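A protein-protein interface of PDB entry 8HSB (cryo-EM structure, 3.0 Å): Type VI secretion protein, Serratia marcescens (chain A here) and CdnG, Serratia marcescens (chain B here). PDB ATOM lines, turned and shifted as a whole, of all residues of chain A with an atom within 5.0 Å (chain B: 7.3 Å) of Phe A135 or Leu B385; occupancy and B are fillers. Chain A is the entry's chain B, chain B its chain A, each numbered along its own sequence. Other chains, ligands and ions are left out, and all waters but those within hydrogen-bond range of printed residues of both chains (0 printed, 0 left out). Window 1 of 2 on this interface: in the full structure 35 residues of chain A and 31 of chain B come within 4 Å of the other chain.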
ATOM      1  N   GLN A  47     -21.106 -15.628 -22.231  1.00  0.00           N
ATOM      2  CA  GLN A  47     -21.625 -14.299 -21.970  1.00  0.00           C
ATOM      3  C   GLN A  47     -21.430 -13.418 -23.195  1.00  0.00           C
ATOM      4  O   GLN A  47     -20.286 -13.208 -23.625  1.00  0.00           O
ATOM      5  CB  GLN A  47     -20.928 -13.669 -20.752  1.00  0.00           C
ATOM      6  CG  GLN A  47     -21.712 -12.542 -20.102  1.00  0.00           C
ATOM      7  CD  GLN A  47     -21.068 -12.045 -18.826  1.00  0.00           C
ATOM      8  OE1 GLN A  47     -20.034 -12.558 -18.399  1.00  0.00           O
ATOM      9  NE2 GLN A  47     -21.677 -11.041 -18.208  1.00  0.00           N
ATOM     10  N   PRO A  48     -22.505 -12.900 -23.794  1.00  0.00           N
ATOM     11  CA  PRO A  48     -22.333 -12.039 -24.977  1.00  0.00           C
ATOM     12  C   PRO A  48     -21.565 -10.758 -24.696  1.00  0.00           C
ATOM     13  O   PRO A  48     -20.535 -10.509 -25.333  1.00  0.00           O
ATOM     14  CB  PRO A  48     -23.780 -11.747 -25.400  1.00  0.00           C
ATOM     15  CG  PRO A  48     -24.572 -12.880 -24.838  1.00  0.00           C
ATOM     16  CD  PRO A  48     -23.922 -13.195 -23.528  1.00  0.00           C
ATOM     17  N   SER A  49     -22.032  -9.943 -23.753  1.00  0.00           N
ATOM     18  CA  SER A  49     -21.452  -8.632 -23.500  1.00  0.00           C
ATOM     19  C   SER A  49     -21.094  -8.508 -22.027  1.00  0.00           C
ATOM     20  O   SER A  49     -21.309  -9.424 -21.229  1.00  0.00           O
ATOM     21  CB  SER A  49     -22.407  -7.507 -23.915  1.00  0.00           C
ATOM     22  OG  SER A  49     -21.949  -6.252 -23.442  1.00  0.00           O
ATOM     23  N   PRO A 128     -18.587 -18.765 -31.434  1.00  0.00           N
ATOM     24  CA  PRO A 128     -18.801 -17.335 -31.724  1.00  0.00           C
ATOM     25  C   PRO A 128     -20.111 -17.063 -32.435  1.00  0.00           C
ATOM     26  O   PRO A 128     -20.727 -16.017 -32.205  1.00  0.00           O
ATOM     27  CB  PRO A 128     -17.591 -16.968 -32.595  1.00  0.00           C
ATOM     28  CG  PRO A 128     -16.568 -17.973 -32.268  1.00  0.00           C
ATOM     29  CD  PRO A 128     -17.318 -19.237 -32.017  1.00  0.00           C
ATOM     30  N   SER A 131     -22.725 -17.001 -29.698  1.00  0.00           N
ATOM     31  CA  SER A 131     -22.625 -15.782 -28.895  1.00  0.00           C
ATOM     32  C   SER A 131     -23.142 -14.568 -29.663  1.00  0.00           C
ATOM     33  O   SER A 131     -23.853 -13.719 -29.105  1.00  0.00           O
ATOM     34  CB  SER A 131     -21.179 -15.567 -28.448  1.00  0.00           C
ATOM     35  OG  SER A 131     -21.033 -14.329 -27.774  1.00  0.00           O
ATOM     36  N   LEU A 132     -22.807 -14.476 -30.951  1.00  0.00           N
ATOM     37  CA  LEU A 132     -23.277 -13.362 -31.764  1.00  0.00           C
ATOM     38  C   LEU A 132     -24.785 -13.432 -31.965  1.00  0.00           C
ATOM     39  O   LEU A 132     -25.461 -12.398 -32.012  1.00  0.00           O
ATOM     40  CB  LEU A 132     -22.545 -13.358 -33.105  1.00  0.00           C
ATOM     41  CG  LEU A 132     -22.860 -12.226 -34.081  1.00  0.00           C
ATOM     42  CD1 LEU A 132     -22.577 -10.883 -33.428  1.00  0.00           C
ATOM     43  CD2 LEU A 132     -22.049 -12.390 -35.352  1.00  0.00           C
ATOM     44  N   TRP A 133     -25.332 -14.645 -32.089  1.00  0.00           N
ATOM     45  CA  TRP A 133     -26.781 -14.804 -32.143  1.00  0.00           C
ATOM     46  C   TRP A 133     -27.429 -14.311 -30.856  1.00  0.00           C
ATOM     47  O   TRP A 133     -28.453 -13.621 -30.890  1.00  0.00           O
ATOM     48  CB  TRP A 133     -27.136 -16.271 -32.399  1.00  0.00           C
ATOM     49  CG  TRP A 133     -28.540 -16.487 -32.894  1.00  0.00           C
ATOM     50  CD1 TRP A 133     -28.922 -16.737 -34.180  1.00  0.00           C
ATOM     51  CD2 TRP A 133     -29.743 -16.479 -32.114  1.00  0.00           C
ATOM     52  NE1 TRP A 133     -30.287 -16.881 -34.250  1.00  0.00           N
ATOM     53  CE2 TRP A 133     -30.814 -16.727 -32.995  1.00  0.00           C
ATOM     54  CE3 TRP A 133     -30.019 -16.286 -30.757  1.00  0.00           C
ATOM     55  CZ2 TRP A 133     -32.136 -16.785 -32.563  1.00  0.00           C
ATOM     56  CZ3 TRP A 133     -31.332 -16.344 -30.333  1.00  0.00           C
ATOM     57  CH2 TRP A 133     -32.374 -16.590 -31.232  1.00  0.00           C
ATOM     58  N   LEU A 134     -26.836 -14.653 -29.709  1.00  0.00           N
ATOM     59  CA  LEU A 134     -27.396 -14.230 -28.430  1.00  0.00           C
ATOM     60  C   LEU A 134     -27.344 -12.714 -28.278  1.00  0.00           C
ATOM     61  O   LEU A 134     -28.232 -12.114 -27.655  1.00  0.00           O
ATOM     62  CB  LEU A 134     -26.657 -14.920 -27.282  1.00  0.00           C
ATOM     63  CG  LEU A 134     -26.911 -16.426 -27.151  1.00  0.00           C
ATOM     64  CD1 LEU A 134     -25.815 -17.107 -26.341  1.00  0.00           C
ATOM     65  CD2 LEU A 134     -28.277 -16.697 -26.540  1.00  0.00           C
ATOM     66  N   PHE A 135     -26.316 -12.075 -28.841  1.00  0.00           N
ATOM     67  CA  PHE A 135     -26.255 -10.616 -28.763  1.00  0.00           C
ATOM     68  C   PHE A 135     -27.439  -9.964 -29.467  1.00  0.00           C
ATOM     69  O   PHE A 135     -28.039  -9.021 -28.938  1.00  0.00           O
ATOM     70  CB  PHE A 135     -24.954 -10.075 -29.350  1.00  0.00           C
ATOM     71  CG  PHE A 135     -24.846  -8.580 -29.247  1.00  0.00           C
ATOM     72  CD1 PHE A 135     -24.543  -7.978 -28.035  1.00  0.00           C
ATOM     73  CD2 PHE A 135     -25.103  -7.773 -30.341  1.00  0.00           C
ATOM     74  CE1 PHE A 135     -24.463  -6.604 -27.926  1.00  0.00           C
ATOM     75  CE2 PHE A 135     -25.033  -6.399 -30.237  1.00  0.00           C
ATOM     76  CZ  PHE A 135     -24.707  -5.813 -29.030  1.00  0.00           C
ATOM     77  N   TYR A 136     -27.778 -10.428 -30.671  1.00  0.00           N
ATOM     78  CA  TYR A 136     -28.926  -9.852 -31.364  1.00  0.00           C
ATOM     79  C   TYR A 136     -30.231 -10.279 -30.708  1.00  0.00           C
ATOM     80  O   TYR A 136     -31.227  -9.549 -30.758  1.00  0.00           O
ATOM     81  CB  TYR A 136     -28.907 -10.237 -32.843  1.00  0.00           C
ATOM     82  CG  TYR A 136     -27.768  -9.610 -33.613  1.00  0.00           C
ATOM     83  CD1 TYR A 136     -27.823  -8.280 -34.010  1.00  0.00           C
ATOM     84  CD2 TYR A 136     -26.644 -10.345 -33.950  1.00  0.00           C
ATOM     85  CE1 TYR A 136     -26.784  -7.700 -34.715  1.00  0.00           C
ATOM     86  CE2 TYR A 136     -25.601  -9.773 -34.654  1.00  0.00           C
ATOM     87  CZ  TYR A 136     -25.675  -8.451 -35.035  1.00  0.00           C
ATOM     88  OH  TYR A 136     -24.638  -7.880 -35.737  1.00  0.00           O
ATOM     89  N   PHE A 137     -30.238 -11.451 -30.069  1.00  0.00           N
ATOM     90  CA  PHE A 137     -31.416 -11.868 -29.316  1.00  0.00           C
ATOM     91  C   PHE A 137     -31.720 -10.894 -28.187  1.00  0.00           C
ATOM     92  O   PHE A 137     -32.877 -10.504 -27.989  1.00  0.00           O
ATOM     93  CB  PHE A 137     -31.215 -13.276 -28.762  1.00  0.00           C
ATOM     94  CG  PHE A 137     -32.092 -13.591 -27.588  1.00  0.00           C
ATOM     95  CD1 PHE A 137     -33.462 -13.708 -27.742  1.00  0.00           C
ATOM     96  CD2 PHE A 137     -31.548 -13.766 -26.327  1.00  0.00           C
ATOM     97  CE1 PHE A 137     -34.272 -13.992 -26.662  1.00  0.00           C
ATOM     98  CE2 PHE A 137     -32.354 -14.051 -25.244  1.00  0.00           C
ATOM     99  CZ  PHE A 137     -33.717 -14.165 -25.412  1.00  0.00           C
ATOM    100  N   GLU A 138     -30.697 -10.486 -27.435  1.00  0.00           N
ATOM    101  CA  GLU A 138     -30.941  -9.558 -26.333  1.00  0.00           C
ATOM    102  C   GLU A 138     -31.209  -8.146 -26.847  1.00  0.00           C
ATOM    103  O   GLU A 138     -31.894  -7.358 -26.184  1.00  0.00           O
ATOM    104  CB  GLU A 138     -29.769  -9.566 -25.351  1.00  0.00           C
ATOM    105  CG  GLU A 138     -28.465  -9.043 -25.908  1.00  0.00           C
ATOM    106  CD  GLU A 138     -27.335  -9.138 -24.908  1.00  0.00           C
ATOM    107  OE1 GLU A 138     -27.574  -9.634 -23.788  1.00  0.00           O
ATOM    108  OE2 GLU A 138     -26.210  -8.710 -25.241  1.00  0.00           O
ATOM    109  N   GLN A 139     -30.675  -7.806 -28.023  1.00  0.00           N
ATOM    110  CA  GLN A 139     -30.929  -6.485 -28.596  1.00  0.00           C
ATOM    111  C   GLN A 139     -32.348  -6.377 -29.141  1.00  0.00           C
ATOM    112  O   GLN A 139     -32.934  -5.286 -29.158  1.00  0.00           O
ATOM    113  CB  GLN A 139     -29.909  -6.179 -29.692  1.00  0.00           C
ATOM    114  CG  GLN A 139     -28.548  -5.753 -29.171  1.00  0.00           C
ATOM    115  CD  GLN A 139     -28.602  -4.431 -28.429  1.00  0.00           C
ATOM    116  OE1 GLN A 139     -28.410  -4.378 -27.215  1.00  0.00           O
ATOM    117  NE2 GLN A 139     -28.869  -3.354 -29.157  1.00  0.00           N
ATOM    118  N   GLU B 340     -28.209  -6.222 -21.525  1.00  0.00           N
ATOM    119  CA  GLU B 340     -27.963  -5.034 -22.336  1.00  0.00           C
ATOM    120  C   GLU B 340     -29.252  -4.272 -22.608  1.00  0.00           C
ATOM    121  O   GLU B 340     -29.218  -3.087 -22.956  1.00  0.00           O
ATOM    122  CB  GLU B 340     -27.277  -5.423 -23.644  1.00  0.00           C
ATOM    123  CG  GLU B 340     -25.805  -5.757 -23.488  1.00  0.00           C
ATOM    124  CD  GLU B 340     -24.934  -4.523 -23.385  1.00  0.00           C
ATOM    125  OE1 GLU B 340     -25.457  -3.406 -23.572  1.00  0.00           O
ATOM    126  OE2 GLU B 340     -23.724  -4.668 -23.114  1.00  0.00           O
ATOM    127  N   PHE B 344     -29.857   0.037 -21.404  1.00  0.00           N
ATOM    128  CA  PHE B 344     -30.360   1.073 -22.297  1.00  0.00           C
ATOM    129  C   PHE B 344     -31.638   1.694 -21.754  1.00  0.00           C
ATOM    130  O   PHE B 344     -31.849   2.901 -21.893  1.00  0.00           O
ATOM    131  CB  PHE B 344     -30.585   0.502 -23.695  1.00  0.00           C
ATOM    132  CG  PHE B 344     -29.316   0.131 -24.406  1.00  0.00           C
ATOM    133  CD1 PHE B 344     -28.153   0.852 -24.193  1.00  0.00           C
ATOM    134  CD2 PHE B 344     -29.287  -0.931 -25.291  1.00  0.00           C
ATOM    135  CE1 PHE B 344     -26.983   0.518 -24.842  1.00  0.00           C
ATOM    136  CE2 PHE B 344     -28.120  -1.271 -25.946  1.00  0.00           C
ATOM    137  CZ  PHE B 344     -26.966  -0.544 -25.720  1.00  0.00           C
ATOM    138  N   LEU B 363     -23.107   2.239 -32.057  1.00  0.00           N
ATOM    139  CA  LEU B 363     -22.519   0.980 -31.598  1.00  0.00           C
ATOM    140  C   LEU B 363     -22.877  -0.170 -32.534  1.00  0.00           C
ATOM    141  O   LEU B 363     -22.019  -0.991 -32.895  1.00  0.00           O
ATOM    142  CB  LEU B 363     -22.986   0.679 -30.174  1.00  0.00           C
ATOM    143  CG  LEU B 363     -22.772  -0.750 -29.670  1.00  0.00           C
ATOM    144  CD1 LEU B 363     -21.325  -0.974 -29.257  1.00  0.00           C
ATOM    145  CD2 LEU B 363     -23.722  -1.051 -28.521  1.00  0.00           C
ATOM    146  N   MET B 364     -24.148  -0.249 -32.936  1.00  0.00           N
ATOM    147  CA  MET B 364     -24.564  -1.317 -33.837  1.00  0.00           C
ATOM    148  C   MET B 364     -23.899  -1.181 -35.199  1.00  0.00           C
ATOM    149  O   MET B 364     -23.492  -2.183 -35.795  1.00  0.00           O
ATOM    150  CB  MET B 364     -26.085  -1.339 -33.981  1.00  0.00           C
ATOM    151  CG  MET B 364     -26.813  -1.696 -32.700  1.00  0.00           C
ATOM    152  SD  MET B 364     -26.360  -3.338 -32.108  1.00  0.00           S
ATOM    153  CE  MET B 364     -27.104  -4.379 -33.356  1.00  0.00           C
ATOM    154  N   MET B 367     -20.252  -2.428 -34.818  1.00  0.00           N
ATOM    155  CA  MET B 367     -20.058  -3.876 -34.759  1.00  0.00           C
ATOM    156  C   MET B 367     -20.506  -4.559 -36.048  1.00  0.00           C
ATOM    157  O   MET B 367     -19.976  -5.617 -36.410  1.00  0.00           O
ATOM    158  CB  MET B 367     -20.755  -4.474 -33.540  1.00  0.00           C
ATOM    159  CG  MET B 367     -20.271  -3.863 -32.236  1.00  0.00           C
ATOM    160  SD  MET B 367     -20.246  -5.027 -30.863  1.00  0.00           S
ATOM    161  CE  MET B 367     -21.865  -5.746 -31.029  1.00  0.00           C
ATOM    162  N   LEU B 376     -14.096  -8.849 -35.539  1.00  0.00           N
ATOM    163  CA  LEU B 376     -14.860  -9.401 -34.426  1.00  0.00           C
ATOM    164  C   LEU B 376     -14.156 -10.661 -33.933  1.00  0.00           C
ATOM    165  O   LEU B 376     -14.237 -11.716 -34.570  1.00  0.00           O
ATOM    166  CB  LEU B 376     -16.295  -9.699 -34.856  1.00  0.00           C
ATOM    167  CG  LEU B 376     -17.388  -9.527 -33.798  1.00  0.00           C
ATOM    168  CD1 LEU B 376     -17.488  -8.077 -33.355  1.00  0.00           C
ATOM    169  CD2 LEU B 376     -18.724 -10.016 -34.329  1.00  0.00           C
ATOM    170  N   HIS B 377     -13.469 -10.551 -32.798  1.00  0.00           N
ATOM    171  CA  HIS B 377     -12.716 -11.658 -32.228  1.00  0.00           C
ATOM    172  C   HIS B 377     -13.507 -12.287 -31.089  1.00  0.00           C
ATOM    173  O   HIS B 377     -14.477 -11.714 -30.586  1.00  0.00           O
ATOM    174  CB  HIS B 377     -11.338 -11.211 -31.719  1.00  0.00           C
ATOM    175  CG  HIS B 377     -10.569 -10.379 -32.697  1.00  0.00           C
ATOM    176  ND1 HIS B 377     -10.320 -10.787 -33.989  1.00  0.00           N
ATOM    177  CD2 HIS B 377      -9.989  -9.162 -32.569  1.00  0.00           C
ATOM    178  CE1 HIS B 377      -9.622  -9.857 -34.616  1.00  0.00           C
ATOM    179  NE2 HIS B 377      -9.408  -8.860 -33.776  1.00  0.00           N
ATOM    180  N   LEU B 378     -13.072 -13.477 -30.685  1.00  0.00           N
ATOM    181  CA  LEU B 378     -13.714 -14.245 -29.625  1.00  0.00           C
ATOM    182  C   LEU B 378     -12.846 -14.200 -28.376  1.00  0.00           C
ATOM    183  O   LEU B 378     -11.659 -14.541 -28.428  1.00  0.00           O
ATOM    184  CB  LEU B 378     -13.940 -15.692 -30.059  1.00  0.00           C
ATOM    185  CG  LEU B 378     -14.695 -16.568 -29.057  1.00  0.00           C
ATOM    186  CD1 LEU B 378     -16.177 -16.220 -29.046  1.00  0.00           C
ATOM    187  CD2 LEU B 378     -14.477 -18.049 -29.345  1.00  0.00           C
ATOM    188  N   ASP B 379     -13.436 -13.781 -27.259  1.00  0.00           N
ATOM    189  CA  ASP B 379     -12.741 -13.839 -25.981  1.00  0.00           C
ATOM    190  C   ASP B 379     -12.527 -15.291 -25.576  1.00  0.00           C
ATOM    191  O   ASP B 379     -13.440 -16.116 -25.677  1.00  0.00           O
ATOM    192  CB  ASP B 379     -13.536 -13.097 -24.908  1.00  0.00           C
ATOM    193  CG  ASP B 379     -13.201 -11.620 -24.849  1.00  0.00           C
ATOM    194  OD1 ASP B 379     -12.011 -11.273 -24.998  1.00  0.00           O
ATOM    195  OD2 ASP B 379     -14.128 -10.806 -24.658  1.00  0.00           O
ATOM    196  N   THR B 382     -14.712 -15.881 -21.657  1.00  0.00           N
ATOM    197  CA  THR B 382     -16.167 -15.835 -21.645  1.00  0.00           C
ATOM    198  C   THR B 382     -16.802 -15.974 -23.021  1.00  0.00           C
ATOM    199  O   THR B 382     -18.034 -16.013 -23.110  1.00  0.00           O
ATOM    200  CB  THR B 382     -16.658 -14.526 -21.008  1.00  0.00           C
ATOM    201  OG1 THR B 382     -16.308 -13.420 -21.849  1.00  0.00           O
ATOM    202  CG2 THR B 382     -16.034 -14.332 -19.636  1.00  0.00           C
ATOM    203  N   GLY B 383     -16.010 -16.047 -24.087  1.00  0.00           N
ATOM    204  CA  GLY B 383     -16.583 -16.120 -25.419  1.00  0.00           C
ATOM    205  C   GLY B 383     -17.311 -14.863 -25.837  1.00  0.00           C
ATOM    206  O   GLY B 383     -18.150 -14.907 -26.743  1.00  0.00           O
ATOM    207  N   GLY B 384     -17.014 -13.735 -25.194  1.00  0.00           N
ATOM    208  CA  GLY B 384     -17.709 -12.505 -25.512  1.00  0.00           C
ATOM    209  C   GLY B 384     -17.245 -11.904 -26.824  1.00  0.00           C
ATOM    210  O   GLY B 384     -16.180 -12.230 -27.350  1.00  0.00           O
ATOM    211  N   LEU B 385     -18.072 -11.011 -27.360  1.00  0.00           N
ATOM    212  CA  LEU B 385     -17.743 -10.339 -28.608  1.00  0.00           C
ATOM    213  C   LEU B 385     -16.677  -9.274 -28.376  1.00  0.00           C
ATOM    214  O   LEU B 385     -16.716  -8.539 -27.385  1.00  0.00           O
ATOM    215  CB  LEU B 385     -18.994  -9.705 -29.212  1.00  0.00           C
ATOM    216  CG  LEU B 385     -20.138 -10.657 -29.567  1.00  0.00           C
ATOM    217  CD1 LEU B 385     -21.358  -9.877 -30.023  1.00  0.00           C
ATOM    218  CD2 LEU B 385     -19.701 -11.649 -30.633  1.00  0.00           C
ATOM    219  N   ILE B 386     -15.722  -9.196 -29.297  1.00  0.00           N
ATOM    220  CA  ILE B 386     -14.662  -8.194 -29.258  1.00  0.00           C
ATOM    221  C   ILE B 386     -14.786  -7.340 -30.510  1.00  0.00           C
ATOM    222  O   ILE B 386     -14.637  -7.844 -31.629  1.00  0.00           O
ATOM    223  CB  ILE B 386     -13.268  -8.834 -29.170  1.00  0.00           C
ATOM    224  CG1 ILE B 386     -13.234  -9.898 -28.074  1.00  0.00           C
ATOM    225  CG2 ILE B 386     -12.209  -7.771 -28.919  1.00  0.00           C
ATOM    226  CD1 ILE B 386     -12.040 -10.817 -28.164  1.00  0.00           C
ATOM    227  N   ALA B 387     -15.052  -6.050 -30.322  1.00  0.00           N
ATOM    228  CA  ALA B 387     -15.215  -5.111 -31.422  1.00  0.00           C
ATOM    229  C   ALA B 387     -13.999  -4.199 -31.490  1.00  0.00           C
ATOM    230  O   ALA B 387     -13.698  -3.486 -30.527  1.00  0.00           O
ATOM    231  CB  ALA B 387     -16.493  -4.283 -31.258  1.00  0.00           C
ATOM    232  N   VAL B 399     -14.790 -13.650 -37.084  1.00  0.00           N
ATOM    233  CA  VAL B 399     -15.962 -14.509 -37.285  1.00  0.00           C
ATOM    234  C   VAL B 399     -16.259 -14.613 -38.777  1.00  0.00           C
ATOM    235  O   VAL B 399     -16.373 -13.577 -39.459  1.00  0.00           O
ATOM    236  CB  VAL B 399     -17.176 -13.953 -36.521  1.00  0.00           C
ATOM    237  CG1 VAL B 399     -18.315 -14.957 -36.539  1.00  0.00           C
ATOM    238  CG2 VAL B 399     -16.787 -13.606 -35.095  1.00  0.00           C
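The side-chain carboxylate of Glu B340 lies within hydrogen-bond range of the side-chain hydroxyl of Ser A49, 2.4 Å away. The backbone carbonyl oxygen (O) of Gly B383 lies within hydrogen-bond range of the side-chain hydroxyl (OG) of Ser A131, at 3.1 Å. O of Thr B382 lies within hydrogen-bond range of N of Gln A47, at 3.2 Å. The backbone carbonyl oxygen (O) of Pro A48 sits at hydrogen-bond distance from the backbone NH (N) of Leu B385, at 3.2 Å.
Of the printed residues of chain B, Phe A135 touches Met B364, Met B367 and Leu B385. Of the printed residues of chain B, Ser A49 touches Glu B340 (2.4 Å). Of the printed residues of chain A, Leu B378 touches Pro A128. Ile B386 touches none of the printed residues of chain A. Trp A133 touches none of the printed residues of chain B. The nearest residue of chain B that does not touch Phe A135 is Glu B340 (4.7 Å). The nearest printed residue of chain A that does not touch Met B364 is Leu A132 (7.9 Å).
Among the printed residues, merely in contact across the chains: Gln A47 with Gly B384 (3.3 Å), Pro A48 with Gly B384 (3.5 Å), Pro A128 with Leu B378 (3.6 Å), Leu A132 with Leu B385 (3.8 Å), Phe A135 with Met B364 (3.8 Å), Phe A135 with Met B367 (3.3 Å), Phe A135 with Leu B385 (3.7 Å), Tyr A136 with Met B364 (3.6 Å), Glu A138 with Glu B340 (3.5 Å), Gln A139 with Glu B340 (3.9 Å), Gln A139 with Phe B344 (3.4 Å) and Gln A139 with Met B364 (3.9 Å).
Hydrophobic or aromatic side chains of chain B that line the printed part of chain A: Phe B344, Met B364, Met B367, Leu B378 and Leu B385. Printed residues of chain A that touch a printed residue of chain B: Gln A47, Pro A48, Ser A49, Pro A128, Ser A131, Leu A132, Phe A135, Tyr A136, Glu A138 and Gln A139. Hydrophobic or aromatic side chains of chain A within 4 Å of the printed part of chain B: Pro A128, Leu A132, Phe A135 and Tyr A136.
The backbone carbonyl oxygen (O) of Gly B384 sits at hydrogen-bond distance from the backbone NH (N) of Asp B379, 3.2 Å away. The side-chain hydroxyl (OG1) of Thr B382 lies close to the backbone NH (N) of Gly B384 (3.4 Å). The side-chain amide nitrogen of Gln A47 sits close to the backbone carbonyl oxygen of Ser A49, at 3.4 Å.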
